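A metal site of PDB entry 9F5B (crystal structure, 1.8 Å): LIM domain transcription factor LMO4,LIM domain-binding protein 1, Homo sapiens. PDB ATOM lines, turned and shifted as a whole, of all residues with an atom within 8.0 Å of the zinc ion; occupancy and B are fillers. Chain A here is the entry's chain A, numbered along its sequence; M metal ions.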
ATOM      1  N   LYS A  34     -13.445  13.182 -15.002  1.00  0.00           N
ATOM      2  CA  LYS A  34     -12.844  13.602 -13.737  1.00  0.00           C
ATOM      3  C   LYS A  34     -11.364  13.932 -13.919  1.00  0.00           C
ATOM      4  O   LYS A  34     -10.668  13.352 -14.772  1.00  0.00           O
ATOM      5  CB  LYS A  34     -12.866  12.491 -12.677  1.00  0.00           C
ATOM      6  CG  LYS A  34     -14.214  12.116 -12.214  1.00  0.00           C
ATOM      7  CD  LYS A  34     -14.174  10.817 -11.388  1.00  0.00           C
ATOM      8  CE  LYS A  34     -14.008   9.568 -12.240  1.00  0.00           C
ATOM      9  NZ  LYS A  34     -14.073   8.270 -11.560  1.00  0.00           N
ATOM     10  N   CYS A  35     -10.877  14.856 -13.087  1.00  0.00           N
ATOM     11  CA  CYS A  35      -9.458  15.149 -13.065  1.00  0.00           C
ATOM     12  C   CYS A  35      -8.674  13.930 -12.596  1.00  0.00           C
ATOM     13  O   CYS A  35      -9.019  13.302 -11.601  1.00  0.00           O
ATOM     14  CB  CYS A  35      -9.185  16.300 -12.115  1.00  0.00           C
ATOM     15  SG  CYS A  35      -7.427  16.728 -12.006  1.00  0.00           S
ATOM     16  N   SER A  36      -7.626  13.589 -13.334  1.00  0.00           N
ATOM     17  CA  SER A  36      -6.771  12.468 -12.990  1.00  0.00           C
ATOM     18  C   SER A  36      -6.138  12.634 -11.604  1.00  0.00           C
ATOM     19  O   SER A  36      -5.900  11.663 -10.892  1.00  0.00           O
ATOM     20  CB  SER A  36      -5.665  12.324 -14.032  1.00  0.00           C
ATOM     21  OG  SER A  36      -6.221  12.007 -15.292  1.00  0.00           O
ATOM     22  N   SER A  37      -5.785  13.870 -11.263  1.00  0.00           N
ATOM     23  CA  SER A  37      -5.057  14.130 -10.006  1.00  0.00           C
ATOM     24  C   SER A  37      -6.013  14.261  -8.814  1.00  0.00           C
ATOM     25  O   SER A  37      -5.796  13.621  -7.778  1.00  0.00           O
ATOM     26  CB  SER A  37      -4.221  15.374 -10.161  1.00  0.00           C
ATOM     27  OG  SER A  37      -3.564  15.688  -8.942  1.00  0.00           O
ATOM     28  N   CYS A  38      -7.041  15.125  -8.909  1.00  0.00           N
ATOM     29  CA  CYS A  38      -7.849  15.472  -7.739  1.00  0.00           C
ATOM     30  C   CYS A  38      -9.265  14.910  -7.793  1.00  0.00           C
ATOM     31  O   CYS A  38     -10.022  15.074  -6.827  1.00  0.00           O
ATOM     32  CB  CYS A  38      -7.908  16.971  -7.525  1.00  0.00           C
ATOM     33  SG  CYS A  38      -8.994  17.792  -8.745  1.00  0.00           S
ATOM     34  N   GLN A  39      -9.646  14.228  -8.878  1.00  0.00           N
ATOM     35  CA  GLN A  39     -10.941  13.574  -8.975  1.00  0.00           C
ATOM     36  C   GLN A  39     -12.114  14.553  -9.155  1.00  0.00           C
ATOM     37  O   GLN A  39     -13.258  14.129  -9.104  1.00  0.00           O
ATOM     38  CB  GLN A  39     -11.258  12.666  -7.785  1.00  0.00           C
ATOM     39  CG  GLN A  39     -10.494  11.342  -7.822  1.00  0.00           C
ATOM     40  CD  GLN A  39      -9.030  11.550  -7.521  1.00  0.00           C
ATOM     41  OE1 GLN A  39      -8.653  11.983  -6.421  1.00  0.00           O
ATOM     42  NE2 GLN A  39      -8.190  11.252  -8.501  1.00  0.00           N
ATOM     43  N   ALA A  40     -11.864  15.866  -9.317  1.00  0.00           N
ATOM     44  CA  ALA A  40     -12.980  16.817  -9.434  1.00  0.00           C
ATOM     45  C   ALA A  40     -13.823  16.487 -10.674  1.00  0.00           C
ATOM     46  O   ALA A  40     -13.292  15.958 -11.671  1.00  0.00           O
ATOM     47  CB  ALA A  40     -12.466  18.233  -9.563  1.00  0.00           C
ATOM     48  N   GLN A  41     -15.119  16.792 -10.623  1.00  0.00           N
ATOM     49  CA  GLN A  41     -15.980  16.554 -11.775  1.00  0.00           C
ATOM     50  C   GLN A  41     -15.876  17.765 -12.708  1.00  0.00           C
ATOM     51  O   GLN A  41     -16.429  18.860 -12.410  1.00  0.00           O
ATOM     52  CB  GLN A  41     -17.427  16.300 -11.353  1.00  0.00           C
ATOM     53  CG  GLN A  41     -17.574  14.932 -10.679  1.00  0.00           C
ATOM     54  CD  GLN A  41     -19.014  14.550 -10.417  1.00  0.00           C
ATOM     55  OE1 GLN A  41     -19.959  15.210 -10.849  1.00  0.00           O
ATOM     56  NE2 GLN A  41     -19.207  13.455  -9.727  1.00  0.00           N
ATOM     57  N   LEU A  42     -15.126  17.599 -13.809  1.00  0.00           N
ATOM     58  CA  LEU A  42     -14.662  18.720 -14.595  1.00  0.00           C
ATOM     59  C   LEU A  42     -15.811  19.563 -15.143  1.00  0.00           C
ATOM     60  O   LEU A  42     -15.666  20.806 -15.278  1.00  0.00           O
ATOM     61  CB  LEU A  42     -13.768  18.215 -15.741  1.00  0.00           C
ATOM     62  CG  LEU A  42     -12.500  17.551 -15.205  1.00  0.00           C
ATOM     63  CD1 LEU A  42     -11.614  16.976 -16.342  1.00  0.00           C
ATOM     64  CD2 LEU A  42     -11.700  18.561 -14.359  1.00  0.00           C
ATOM     65  N   ILE A  45     -17.048  21.881 -12.207  1.00  0.00           N
ATOM     66  CA  ILE A  45     -16.168  22.862 -11.574  1.00  0.00           C
ATOM     67  C   ILE A  45     -15.767  23.975 -12.547  1.00  0.00           C
ATOM     68  O   ILE A  45     -15.497  25.094 -12.132  1.00  0.00           O
ATOM     69  CB  ILE A  45     -14.951  22.206 -10.905  1.00  0.00           C
ATOM     70  CG1 ILE A  45     -14.036  21.536 -11.920  1.00  0.00           C
ATOM     71  CG2 ILE A  45     -15.416  21.187  -9.876  1.00  0.00           C
ATOM     72  CD1 ILE A  45     -12.596  21.499 -11.482  1.00  0.00           C
ATOM     73  N   ILE A  56      -6.039  13.687 -17.868  1.00  0.00           N
ATOM     74  CA  ILE A  56      -7.101  14.667 -18.110  1.00  0.00           C
ATOM     75  C   ILE A  56      -7.188  15.446 -16.810  1.00  0.00           C
ATOM     76  O   ILE A  56      -7.423  14.857 -15.746  1.00  0.00           O
ATOM     77  CB  ILE A  56      -8.454  14.005 -18.431  1.00  0.00           C
ATOM     78  CG1 ILE A  56      -8.325  13.185 -19.723  1.00  0.00           C
ATOM     79  CG2 ILE A  56      -9.516  15.066 -18.594  1.00  0.00           C
ATOM     80  CD1 ILE A  56      -9.557  12.388 -20.036  1.00  0.00           C
ATOM     81  N   LEU A  57      -6.937  16.758 -16.872  1.00  0.00           N
ATOM     82  CA  LEU A  57      -6.700  17.551 -15.670  1.00  0.00           C
ATOM     83  C   LEU A  57      -7.643  18.749 -15.551  1.00  0.00           C
ATOM     84  O   LEU A  57      -7.976  19.399 -16.560  1.00  0.00           O
ATOM     85  CB  LEU A  57      -5.264  18.054 -15.667  1.00  0.00           C
ATOM     86  CG  LEU A  57      -4.183  16.975 -15.625  1.00  0.00           C
ATOM     87  CD1 LEU A  57      -2.790  17.579 -15.831  1.00  0.00           C
ATOM     88  CD2 LEU A  57      -4.260  16.228 -14.297  1.00  0.00           C
ATOM     89  N   CYS A  58      -7.985  19.106 -14.312  1.00  0.00           N
ATOM     90  CA  CYS A  58      -8.591  20.411 -14.102  1.00  0.00           C
ATOM     91  C   CYS A  58      -7.549  21.501 -14.316  1.00  0.00           C
ATOM     92  O   CYS A  58      -6.348  21.230 -14.411  1.00  0.00           O
ATOM     93  CB  CYS A  58      -9.185  20.526 -12.695  1.00  0.00           C
ATOM     94  SG  CYS A  58      -7.954  20.574 -11.334  1.00  0.00           S
ATOM     95  N   ARG A  59      -7.993  22.756 -14.404  1.00  0.00           N
ATOM     96  CA  ARG A  59      -7.055  23.854 -14.651  1.00  0.00           C
ATOM     97  C   ARG A  59      -6.025  23.968 -13.531  1.00  0.00           C
ATOM     98  O   ARG A  59      -4.825  24.135 -13.790  1.00  0.00           O
ATOM     99  CB  ARG A  59      -7.776  25.193 -14.902  1.00  0.00           C
ATOM    100  CG  ARG A  59      -6.784  26.251 -15.357  1.00  0.00           C
ATOM    101  CD  ARG A  59      -7.546  27.506 -15.798  1.00  0.00           C
ATOM    102  NE  ARG A  59      -6.720  28.567 -16.386  1.00  0.00           N
ATOM    103  CZ  ARG A  59      -6.377  29.623 -15.670  1.00  0.00           C
ATOM    104  NH1 ARG A  59      -6.664  29.641 -14.394  1.00  0.00           N
ATOM    105  NH2 ARG A  59      -5.738  30.646 -16.219  1.00  0.00           N
ATOM    106  N   ASN A  60      -6.463  23.900 -12.281  1.00  0.00           N
ATOM    107  CA  ASN A  60      -5.516  24.084 -11.188  1.00  0.00           C
ATOM    108  C   ASN A  60      -4.430  23.016 -11.171  1.00  0.00           C
ATOM    109  O   ASN A  60      -3.258  23.308 -10.936  1.00  0.00           O
ATOM    110  CB  ASN A  60      -6.282  24.094  -9.866  1.00  0.00           C
ATOM    111  CG  ASN A  60      -7.086  25.372  -9.717  1.00  0.00           C
ATOM    112  OD1 ASN A  60      -6.781  26.405 -10.338  1.00  0.00           O
ATOM    113  ND2 ASN A  60      -8.137  25.321  -8.913  1.00  0.00           N
ATOM    114  N   ASP A  61      -4.797  21.763 -11.436  1.00  0.00           N
ATOM    115  CA  ASP A  61      -3.751  20.739 -11.440  1.00  0.00           C
ATOM    116  C   ASP A  61      -2.895  20.800 -12.692  1.00  0.00           C
ATOM    117  O   ASP A  61      -1.748  20.364 -12.671  1.00  0.00           O
ATOM    118  CB  ASP A  61      -4.349  19.366 -11.235  1.00  0.00           C
ATOM    119  CG  ASP A  61      -4.720  19.137  -9.781  1.00  0.00           C
ATOM    120  OD1 ASP A  61      -3.866  19.360  -8.916  1.00  0.00           O
ATOM    121  OD2 ASP A  61      -5.870  18.778  -9.511  1.00  0.00           O
ATOM    122  N   TYR A  62      -3.455  21.268 -13.822  1.00  0.00           N
ATOM    123  CA  TYR A  62      -2.634  21.480 -14.988  1.00  0.00           C
ATOM    124  C   TYR A  62      -1.573  22.546 -14.694  1.00  0.00           C
ATOM    125  O   TYR A  62      -0.392  22.376 -15.032  1.00  0.00           O
ATOM    126  CB  TYR A  62      -3.473  21.945 -16.176  1.00  0.00           C
ATOM    127  CG  TYR A  62      -2.671  22.227 -17.435  1.00  0.00           C
ATOM    128  CD1 TYR A  62      -2.171  21.190 -18.225  1.00  0.00           C
ATOM    129  CD2 TYR A  62      -2.439  23.543 -17.871  1.00  0.00           C
ATOM    130  CE1 TYR A  62      -1.463  21.443 -19.398  1.00  0.00           C
ATOM    131  CE2 TYR A  62      -1.732  23.805 -19.033  1.00  0.00           C
ATOM    132  CZ  TYR A  62      -1.254  22.760 -19.801  1.00  0.00           C
ATOM    133  OH  TYR A  62      -0.573  22.989 -20.965  1.00  0.00           O
ATOM    134  N   ARG A  64      -0.478  23.406 -11.720  1.00  0.00           N
ATOM    135  CA  ARG A  64       0.425  22.897 -10.699  1.00  0.00           C
ATOM    136  C   ARG A  64       1.465  21.936 -11.293  1.00  0.00           C
ATOM    137  O   ARG A  64       2.637  22.005 -10.946  1.00  0.00           O
ATOM    138  CB  ARG A  64      -0.385  22.179  -9.612  1.00  0.00           C
ATOM    139  CG  ARG A  64       0.479  21.661  -8.470  1.00  0.00           C
ATOM    140  CD  ARG A  64      -0.351  20.965  -7.393  1.00  0.00           C
ATOM    141  NE  ARG A  64      -1.073  19.774  -7.892  1.00  0.00           N
ATOM    142  CZ  ARG A  64      -0.565  18.563  -8.022  1.00  0.00           C
ATOM    143  NH1 ARG A  64       0.696  18.284  -7.672  1.00  0.00           N
ATOM    144  NH2 ARG A  64      -1.348  17.574  -8.459  1.00  0.00           N
ATOM    145  N   LEU A  65       1.044  21.038 -12.194  1.00  0.00           N
ATOM    146  CA  LEU A  65       1.961  20.036 -12.714  1.00  0.00           C
ATOM    147  C   LEU A  65       2.787  20.534 -13.887  1.00  0.00           C
ATOM    148  O   LEU A  65       3.854  19.977 -14.157  1.00  0.00           O
ATOM    149  CB  LEU A  65       1.214  18.754 -13.115  1.00  0.00           C
ATOM    150  CG  LEU A  65       0.597  17.931 -11.983  1.00  0.00           C
ATOM    151  CD1 LEU A  65      -0.306  16.850 -12.530  1.00  0.00           C
ATOM    152  CD2 LEU A  65       1.703  17.322 -11.109  1.00  0.00           C
HETATM  153 ZN    ZN M   1      -7.633  18.483 -10.437  1.00  0.00          ZN
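The zinc ion is bound by OD2 of Asp 61 (2.0 Å).
The side-chain sulfur (SG) of Cys 38 binds the zinc ion, at 2.3 Å.
SG of Cys 58 is bound to the zinc ion.
The side-chain sulfur (SG) of Cys 35 binds the zinc ion, 2.4 Å away.
The backbone NH (N) of Asn 60 lies close to the side-chain sulfur (SG) of Cys 58.
The side-chain sulfur (SG) of Cys 35 sits close to the backbone NH (N) of Ser 37 (3.4 Å).
OD1 of Asp 61 is in salt-bridge range of NE of Arg 64 (3.0 Å).
SG of Cys 38 lies close to N of Ala 40, 3.5 Å away.
The backbone NH (N) of Cys 35 is in hydrogen-bond range of the backbone carbonyl oxygen (O) of Ala 40 (3.0 Å).
Four residues have an atom within 4 Å of the zinc ion: Cys 35, Cys 38, Cys 58 and Asp 61.
The nearest printed residue that does not touch the zinc ion is Ser 37 (4.6 Å).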
